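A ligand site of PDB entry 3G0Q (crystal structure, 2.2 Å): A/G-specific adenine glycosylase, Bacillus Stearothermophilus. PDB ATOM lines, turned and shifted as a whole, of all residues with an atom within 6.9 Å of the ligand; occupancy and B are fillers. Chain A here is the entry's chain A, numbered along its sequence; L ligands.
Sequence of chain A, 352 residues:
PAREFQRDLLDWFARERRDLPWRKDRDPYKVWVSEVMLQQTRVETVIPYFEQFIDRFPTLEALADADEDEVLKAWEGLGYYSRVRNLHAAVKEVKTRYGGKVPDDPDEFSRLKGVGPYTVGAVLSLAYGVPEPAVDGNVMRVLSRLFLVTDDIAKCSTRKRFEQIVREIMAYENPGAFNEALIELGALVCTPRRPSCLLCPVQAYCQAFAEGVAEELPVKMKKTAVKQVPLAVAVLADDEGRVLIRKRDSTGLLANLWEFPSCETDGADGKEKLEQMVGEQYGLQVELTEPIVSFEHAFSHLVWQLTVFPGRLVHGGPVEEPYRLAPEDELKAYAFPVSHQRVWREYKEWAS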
ATOM      1  N   ARG A 141      -1.383 -25.501  19.321  1.00  0.00           N
ATOM      2  CA  ARG A 141      -0.702 -26.143  18.215  1.00  0.00           C
ATOM      3  C   ARG A 141      -1.275 -25.610  16.909  1.00  0.00           C
ATOM      4  O   ARG A 141      -0.544 -25.276  15.995  1.00  0.00           O
ATOM      5  CB  ARG A 141      -0.869 -27.665  18.292  1.00  0.00           C
ATOM      6  CG  ARG A 141      -0.126 -28.411  17.201  1.00  0.00           C
ATOM      7  CD  ARG A 141      -0.128 -29.919  17.459  1.00  0.00           C
ATOM      8  NE  ARG A 141      -1.486 -30.428  17.437  1.00  0.00           N
ATOM      9  CZ  ARG A 141      -2.184 -30.747  18.522  1.00  0.00           C
ATOM     10  NH1 ARG A 141      -1.649 -30.619  19.728  1.00  0.00           N
ATOM     11  NH2 ARG A 141      -3.430 -31.183  18.386  1.00  0.00           N
ATOM     12  N   VAL A 142      -2.600 -25.515  16.849  1.00  0.00           N
ATOM     13  CA  VAL A 142      -3.219 -25.017  15.634  1.00  0.00           C
ATOM     14  C   VAL A 142      -2.789 -23.607  15.300  1.00  0.00           C
ATOM     15  O   VAL A 142      -2.324 -23.341  14.193  1.00  0.00           O
ATOM     16  CB  VAL A 142      -4.759 -25.033  15.734  1.00  0.00           C
ATOM     17  CG1 VAL A 142      -5.359 -24.316  14.528  1.00  0.00           C
ATOM     18  CG2 VAL A 142      -5.267 -26.472  15.792  1.00  0.00           C
ATOM     19  N   LEU A 143      -2.953 -22.700  16.263  1.00  0.00           N
ATOM     20  CA  LEU A 143      -2.598 -21.306  16.030  1.00  0.00           C
ATOM     21  C   LEU A 143      -1.120 -21.163  15.759  1.00  0.00           C
ATOM     22  O   LEU A 143      -0.713 -20.375  14.905  1.00  0.00           O
ATOM     23  CB  LEU A 143      -3.025 -20.444  17.223  1.00  0.00           C
ATOM     24  CG  LEU A 143      -4.518 -20.325  17.529  1.00  0.00           C
ATOM     25  CD1 LEU A 143      -4.708 -19.420  18.751  1.00  0.00           C
ATOM     26  CD2 LEU A 143      -5.280 -19.780  16.343  1.00  0.00           C
ATOM     27  N   ARG A 145       0.779 -23.088  14.186  1.00  0.00           N
ATOM     28  CA  ARG A 145       1.038 -23.453  12.810  1.00  0.00           C
ATOM     29  C   ARG A 145       0.417 -22.473  11.814  1.00  0.00           C
ATOM     30  O   ARG A 145       1.064 -22.088  10.840  1.00  0.00           O
ATOM     31  CB  ARG A 145       0.531 -24.878  12.548  1.00  0.00           C
ATOM     32  CG  ARG A 145       1.415 -25.964  13.149  1.00  0.00           C
ATOM     33  CD  ARG A 145       0.685 -27.290  13.284  1.00  0.00           C
ATOM     34  NE  ARG A 145       1.598 -28.353  13.731  1.00  0.00           N
ATOM     35  CZ  ARG A 145       1.229 -29.601  13.981  1.00  0.00           C
ATOM     36  NH1 ARG A 145      -0.047 -29.974  13.843  1.00  0.00           N
ATOM     37  NH2 ARG A 145       2.139 -30.504  14.361  1.00  0.00           N
ATOM     38  N   LEU A 146      -0.817 -22.063  12.063  1.00  0.00           N
ATOM     39  CA  LEU A 146      -1.494 -21.130  11.165  1.00  0.00           C
ATOM     40  C   LEU A 146      -0.769 -19.788  11.036  1.00  0.00           C
ATOM     41  O   LEU A 146      -0.608 -19.265   9.931  1.00  0.00           O
ATOM     42  CB  LEU A 146      -2.926 -20.864  11.630  1.00  0.00           C
ATOM     43  CG  LEU A 146      -4.034 -21.893  11.404  1.00  0.00           C
ATOM     44  CD1 LEU A 146      -5.321 -21.380  12.027  1.00  0.00           C
ATOM     45  CD2 LEU A 146      -4.245 -22.137   9.919  1.00  0.00           C
ATOM     46  N   LEU A 185     -10.379 -29.315  15.415  1.00  0.00           N
ATOM     47  CA  LEU A 185      -9.409 -29.312  14.318  1.00  0.00           C
ATOM     48  C   LEU A 185      -8.082 -29.831  14.830  1.00  0.00           C
ATOM     49  O   LEU A 185      -7.425 -30.655  14.187  1.00  0.00           O
ATOM     50  CB  LEU A 185      -9.183 -27.902  13.756  1.00  0.00           C
ATOM     51  CG  LEU A 185      -8.245 -27.886  12.547  1.00  0.00           C
ATOM     52  CD1 LEU A 185      -8.963 -28.541  11.381  1.00  0.00           C
ATOM     53  CD2 LEU A 185      -7.821 -26.469  12.173  1.00  0.00           C
ATOM     54  N   VAL A 189      -7.418 -33.201  12.823  1.00  0.00           N
ATOM     55  CA  VAL A 189      -6.647 -32.925  11.630  1.00  0.00           C
ATOM     56  C   VAL A 189      -5.237 -32.410  11.890  1.00  0.00           C
ATOM     57  O   VAL A 189      -4.252 -33.034  11.466  1.00  0.00           O
ATOM     58  CB  VAL A 189      -7.392 -31.887  10.741  1.00  0.00           C
ATOM     59  CG1 VAL A 189      -6.559 -31.543   9.515  1.00  0.00           C
ATOM     60  CG2 VAL A 189      -8.738 -32.456  10.323  1.00  0.00           C
ATOM     61  N   CYS A 190      -5.153 -31.282  12.587  1.00  0.00           N
ATOM     62  CA  CYS A 190      -3.875 -30.636  12.897  1.00  0.00           C
ATOM     63  C   CYS A 190      -3.271 -31.267  14.152  1.00  0.00           C
ATOM     64  O   CYS A 190      -3.136 -30.622  15.200  1.00  0.00           O
ATOM     65  CB  CYS A 190      -4.140 -29.143  13.086  1.00  0.00           C
ATOM     66  SG  CYS A 190      -2.680 -28.135  13.134  1.00  0.00           S
ATOM     67  N   THR A 191      -2.886 -32.537  14.007  1.00  0.00           N
ATOM     68  CA  THR A 191      -2.346 -33.359  15.078  1.00  0.00           C
ATOM     69  C   THR A 191      -0.891 -33.132  15.415  1.00  0.00           C
ATOM     70  O   THR A 191      -0.145 -32.578  14.608  1.00  0.00           O
ATOM     71  CB  THR A 191      -2.559 -34.866  14.737  1.00  0.00           C
ATOM     72  OG1 THR A 191      -2.008 -35.139  13.442  1.00  0.00           O
ATOM     73  CG2 THR A 191      -4.052 -35.193  14.710  1.00  0.00           C
ATOM     74  N   PRO A 195       0.353 -33.981  10.732  1.00  0.00           N
ATOM     75  CA  PRO A 195      -0.997 -33.443  10.583  1.00  0.00           C
ATOM     76  C   PRO A 195      -1.475 -33.725   9.172  1.00  0.00           C
ATOM     77  O   PRO A 195      -0.661 -33.945   8.280  1.00  0.00           O
ATOM     78  CB  PRO A 195      -0.792 -31.956  10.844  1.00  0.00           C
ATOM     79  CG  PRO A 195       0.578 -31.723  10.284  1.00  0.00           C
ATOM     80  CD  PRO A 195       1.348 -32.903  10.837  1.00  0.00           C
ATOM     81  N   SER A 196      -2.777 -33.713   8.956  1.00  0.00           N
ATOM     82  CA  SER A 196      -3.351 -33.992   7.648  1.00  0.00           C
ATOM     83  C   SER A 196      -3.635 -32.713   6.876  1.00  0.00           C
ATOM     84  O   SER A 196      -4.785 -32.434   6.505  1.00  0.00           O
ATOM     85  CB  SER A 196      -4.619 -34.826   7.809  1.00  0.00           C
ATOM     86  OG  SER A 196      -4.295 -36.084   8.379  1.00  0.00           O
ATOM     87  N   CYS A 197      -2.582 -31.955   6.627  1.00  0.00           N
ATOM     88  CA  CYS A 197      -2.666 -30.690   5.915  1.00  0.00           C
ATOM     89  C   CYS A 197      -3.369 -30.795   4.548  1.00  0.00           C
ATOM     90  O   CYS A 197      -4.107 -29.887   4.161  1.00  0.00           O
ATOM     91  CB  CYS A 197      -1.258 -30.097   5.747  1.00  0.00           C
ATOM     92  SG  CYS A 197      -0.277 -29.956   7.311  1.00  0.00           S
ATOM     93  N   LEU A 198      -3.167 -31.889   3.816  1.00  0.00           N
ATOM     94  CA  LEU A 198      -3.815 -32.047   2.506  1.00  0.00           C
ATOM     95  C   LEU A 198      -5.341 -32.116   2.632  1.00  0.00           C
ATOM     96  O   LEU A 198      -6.056 -31.845   1.674  1.00  0.00           O
ATOM     97  CB  LEU A 198      -3.314 -33.309   1.808  1.00  0.00           C
ATOM     98  CG  LEU A 198      -1.793 -33.426   1.638  1.00  0.00           C
ATOM     99  CD1 LEU A 198      -1.419 -34.780   1.075  1.00  0.00           C
ATOM    100  CD2 LEU A 198      -1.315 -32.306   0.736  1.00  0.00           C
ATOM    101  N   LEU A 199      -5.827 -32.516   3.804  1.00  0.00           N
ATOM    102  CA  LEU A 199      -7.261 -32.623   4.024  1.00  0.00           C
ATOM    103  C   LEU A 199      -7.771 -31.553   4.992  1.00  0.00           C
ATOM    104  O   LEU A 199      -8.927 -31.566   5.400  1.00  0.00           O
ATOM    105  CB  LEU A 199      -7.600 -34.013   4.593  1.00  0.00           C
ATOM    106  CG  LEU A 199      -7.279 -35.257   3.752  1.00  0.00           C
ATOM    107  CD1 LEU A 199      -7.479 -36.513   4.599  1.00  0.00           C
ATOM    108  CD2 LEU A 199      -8.157 -35.301   2.510  1.00  0.00           C
ATOM    109  N   CYS A 200      -6.892 -30.626   5.362  1.00  0.00           N
ATOM    110  CA  CYS A 200      -7.283 -29.577   6.300  1.00  0.00           C
ATOM    111  C   CYS A 200      -8.198 -28.543   5.661  1.00  0.00           C
ATOM    112  O   CYS A 200      -7.931 -28.061   4.561  1.00  0.00           O
ATOM    113  CB  CYS A 200      -6.031 -28.875   6.858  1.00  0.00           C
ATOM    114  SG  CYS A 200      -6.410 -27.548   8.026  1.00  0.00           S
ATOM    115  N   PRO A 201      -9.299 -28.193   6.342  1.00  0.00           N
ATOM    116  CA  PRO A 201     -10.264 -27.215   5.823  1.00  0.00           C
ATOM    117  C   PRO A 201      -9.784 -25.764   5.914  1.00  0.00           C
ATOM    118  O   PRO A 201     -10.494 -24.860   5.484  1.00  0.00           O
ATOM    119  CB  PRO A 201     -11.498 -27.472   6.676  1.00  0.00           C
ATOM    120  CG  PRO A 201     -10.872 -27.828   8.020  1.00  0.00           C
ATOM    121  CD  PRO A 201      -9.770 -28.796   7.601  1.00  0.00           C
ATOM    122  N   VAL A 202      -8.608 -25.537   6.484  1.00  0.00           N
ATOM    123  CA  VAL A 202      -8.114 -24.167   6.561  1.00  0.00           C
ATOM    124  C   VAL A 202      -6.675 -24.097   6.095  1.00  0.00           C
ATOM    125  O   VAL A 202      -5.924 -23.211   6.466  1.00  0.00           O
ATOM    126  CB  VAL A 202      -8.243 -23.603   7.996  1.00  0.00           C
ATOM    127  CG1 VAL A 202      -9.720 -23.508   8.370  1.00  0.00           C
ATOM    128  CG2 VAL A 202      -7.494 -24.477   8.992  1.00  0.00           C
ATOM    129  N   GLN A 203      -6.317 -25.068   5.255  1.00  0.00           N
ATOM    130  CA  GLN A 203      -4.983 -25.158   4.676  1.00  0.00           C
ATOM    131  C   GLN A 203      -4.591 -23.872   3.960  1.00  0.00           C
ATOM    132  O   GLN A 203      -3.474 -23.398   4.082  1.00  0.00           O
ATOM    133  CB  GLN A 203      -4.952 -26.293   3.671  1.00  0.00           C
ATOM    134  CG  GLN A 203      -3.620 -26.527   2.996  1.00  0.00           C
ATOM    135  CD  GLN A 203      -3.767 -27.350   1.714  1.00  0.00           C
ATOM    136  OE1 GLN A 203      -4.162 -26.820   0.668  1.00  0.00           O
ATOM    137  NE2 GLN A 203      -3.482 -28.637   1.794  1.00  0.00           N
ATOM    138  N   ALA A 204      -5.539 -23.321   3.200  1.00  0.00           N
ATOM    139  CA  ALA A 204      -5.292 -22.109   2.429  1.00  0.00           C
ATOM    140  C   ALA A 204      -4.778 -20.972   3.301  1.00  0.00           C
ATOM    141  O   ALA A 204      -3.938 -20.183   2.854  1.00  0.00           O
ATOM    142  CB  ALA A 204      -6.579 -21.691   1.726  1.00  0.00           C
ATOM    143  N   TYR A 205      -5.264 -20.897   4.527  1.00  0.00           N
ATOM    144  CA  TYR A 205      -4.892 -19.835   5.453  1.00  0.00           C
ATOM    145  C   TYR A 205      -3.652 -20.151   6.279  1.00  0.00           C
ATOM    146  O   TYR A 205      -3.195 -19.306   7.041  1.00  0.00           O
ATOM    147  CB  TYR A 205      -6.022 -19.551   6.432  1.00  0.00           C
ATOM    148  CG  TYR A 205      -7.401 -19.418   5.821  1.00  0.00           C
ATOM    149  CD1 TYR A 205      -8.075 -20.533   5.309  1.00  0.00           C
ATOM    150  CD2 TYR A 205      -8.046 -18.188   5.789  1.00  0.00           C
ATOM    151  CE1 TYR A 205      -9.363 -20.416   4.787  1.00  0.00           C
ATOM    152  CE2 TYR A 205      -9.339 -18.056   5.273  1.00  0.00           C
ATOM    153  CZ  TYR A 205      -9.988 -19.175   4.777  1.00  0.00           C
ATOM    154  OH  TYR A 205     -11.269 -19.045   4.288  1.00  0.00           O
ATOM    155  N   CYS A 206      -3.097 -21.351   6.129  1.00  0.00           N
ATOM    156  CA  CYS A 206      -1.953 -21.736   6.952  1.00  0.00           C
ATOM    157  C   CYS A 206      -0.537 -21.388   6.511  1.00  0.00           C
ATOM    158  O   CYS A 206      -0.015 -21.929   5.540  1.00  0.00           O
ATOM    159  CB  CYS A 206      -2.031 -23.230   7.259  1.00  0.00           C
ATOM    160  SG  CYS A 206      -0.784 -23.741   8.435  1.00  0.00           S
ATOM    161  N   GLN A 207       0.105 -20.526   7.294  1.00  0.00           N
ATOM    162  CA  GLN A 207       1.464 -20.103   7.000  1.00  0.00           C
ATOM    163  C   GLN A 207       2.459 -21.238   7.176  1.00  0.00           C
ATOM    164  O   GLN A 207       3.454 -21.325   6.459  1.00  0.00           O
ATOM    165  CB  GLN A 207       1.855 -18.915   7.892  1.00  0.00           C
ATOM    166  CG  GLN A 207       1.163 -17.598   7.548  1.00  0.00           C
ATOM    167  CD  GLN A 207       1.430 -16.524   8.596  1.00  0.00           C
ATOM    168  OE1 GLN A 207       2.577 -16.242   8.925  1.00  0.00           O
ATOM    169  NE2 GLN A 207       0.359 -15.927   9.109  1.00  0.00           N
ATOM    170  N   ALA A 208       2.213 -22.105   8.151  1.00  0.00           N
ATOM    171  CA  ALA A 208       3.130 -23.218   8.370  1.00  0.00           C
ATOM    172  C   ALA A 208       3.130 -24.176   7.174  1.00  0.00           C
ATOM    173  O   ALA A 208       4.159 -24.721   6.799  1.00  0.00           O
ATOM    174  CB  ALA A 208       2.767 -23.970   9.644  1.00  0.00           C
ATOM    175  N   PHE A 209       1.956 -24.410   6.592  1.00  0.00           N
ATOM    176  CA  PHE A 209       1.885 -25.304   5.440  1.00  0.00           C
ATOM    177  C   PHE A 209       2.591 -24.686   4.243  1.00  0.00           C
ATOM    178  O   PHE A 209       3.394 -25.334   3.577  1.00  0.00           O
ATOM    179  CB  PHE A 209       0.434 -25.596   5.061  1.00  0.00           C
ATOM    180  CG  PHE A 209       0.307 -26.509   3.879  1.00  0.00           C
ATOM    181  CD1 PHE A 209       0.694 -27.843   3.976  1.00  0.00           C
ATOM    182  CD2 PHE A 209      -0.142 -26.027   2.646  1.00  0.00           C
ATOM    183  CE1 PHE A 209       0.643 -28.676   2.863  1.00  0.00           C
ATOM    184  CE2 PHE A 209      -0.197 -26.852   1.528  1.00  0.00           C
ATOM    185  CZ  PHE A 209       0.192 -28.187   1.643  1.00  0.00           C
ATOM    186  N   VAL A 213       6.670 -26.186   7.266  1.00  0.00           N
ATOM    187  CA  VAL A 213       7.222 -26.493   8.578  1.00  0.00           C
ATOM    188  C   VAL A 213       6.173 -26.985   9.592  1.00  0.00           C
ATOM    189  O   VAL A 213       6.430 -27.029  10.795  1.00  0.00           O
ATOM    190  CB  VAL A 213       7.923 -25.253   9.199  1.00  0.00           C
ATOM    191  CG1 VAL A 213       9.058 -24.798   8.302  1.00  0.00           C
ATOM    192  CG2 VAL A 213       6.913 -24.122   9.385  1.00  0.00           C
ATOM    193  N   ALA A 214       4.999 -27.348   9.084  1.00  0.00           N
ATOM    194  CA  ALA A 214       3.897 -27.824   9.930  1.00  0.00           C
ATOM    195  C   ALA A 214       4.357 -28.825  10.978  1.00  0.00           C
ATOM    196  O   ALA A 214       3.994 -28.708  12.151  1.00  0.00           O
ATOM    197  CB  ALA A 214       2.799 -28.453   9.060  1.00  0.00           C
ATOM    198  N   GLU A 215       5.163 -29.790  10.561  1.00  0.00           N
ATOM    199  CA  GLU A 215       5.655 -30.833  11.472  1.00  0.00           C
ATOM    200  C   GLU A 215       6.685 -30.386  12.514  1.00  0.00           C
ATOM    201  O   GLU A 215       6.905 -31.099  13.494  1.00  0.00           O
ATOM    202  CB  GLU A 215       6.219 -32.007  10.676  1.00  0.00           C
ATOM    203  CG  GLU A 215       5.246 -32.565   9.643  1.00  0.00           C
ATOM    204  CD  GLU A 215       5.690 -33.889   9.061  1.00  0.00           C
ATOM    205  OE1 GLU A 215       6.837 -33.975   8.589  1.00  0.00           O
ATOM    206  OE2 GLU A 215       4.874 -34.841   9.085  1.00  0.00           O
HETATM  207 FE1  LIG L   1      -1.975 -25.882   8.855  1.00  0.00          FE
HETATM  208 FE2  LIG L   1      -2.590 -27.630  10.730  1.00  0.00          FE
HETATM  209 FE3  LIG L   1      -4.118 -27.493   8.636  1.00  0.00          FE
HETATM  210 FE4  LIG L   1      -1.686 -28.471   8.342  1.00  0.00          FE
HETATM  211  S1  LIG L   1      -3.350 -29.348   9.444  1.00  0.00           S
HETATM  212  S2  LIG L   1      -2.742 -27.032   7.145  1.00  0.00           S
HETATM  213  S3  LIG L   1      -0.575 -27.283   9.853  1.00  0.00           S
HETATM  214  S4  LIG L   1      -3.778 -25.936  10.271  1.00  0.00           S
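O of Leu 185 lies within hydrogen-bond range of N of Cys 190, 2.8 Å away. The backbone carbonyl oxygen (O) of Cys 190 lies within hydrogen-bond range of the guanidinium group (NE) of Arg 141. The side-chain sulfur of Cys 206 lies close to the backbone carbonyl oxygen of Arg 145. N of Phe 209 sits close to SG of Cys 206 (3.4 Å). The backbone carbonyl oxygen (O) of Ala 214 lies within hydrogen-bond range of the guanidinium group (NE) of Arg 145 (2.9 Å). The guanidinium group (NH1) of Arg 145 lies within hydrogen-bond range of the backbone carbonyl oxygen (O) of Thr 191 (2.7 Å). N of Gln 207 sits at hydrogen-bond distance from O of Leu 146. The backbone carbonyl oxygen (O) of Val 189 is in hydrogen-bond range of the backbone NH (N) of Ser 196, 3.0 Å away.
SG of Cys 197 binds FE4 of the ligand, 2.3 Å away. An iron atom (FE3) of the ligand is bound by the side-chain sulfur (SG) of Cys 200, at 2.4 Å. An iron atom (FE2) of the ligand is bound by the side-chain sulfur (SG) of Cys 190, 2.5 Å away. The side-chain sulfur (SG) of Cys 206 is bound to an iron atom (FE1) of the ligand.
CD of Arg 145 touches S3 of the ligand (3.7 Å). CD2 of Leu 146 touches S4 of the ligand, at 3.8 Å. CG1 of Val 189 touches S1 of the ligand, at 3.9 Å. CB of Pro 195 touches S1 of the ligand, 3.9 Å away. CA of Gln 203 touches S2 of the ligand, at 3.8 Å. CB of Ala 214 touches S3 of the ligand, at 3.7 Å. The nearest printed residue that does not touch the ligand is Phe 209 (4.1 Å).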
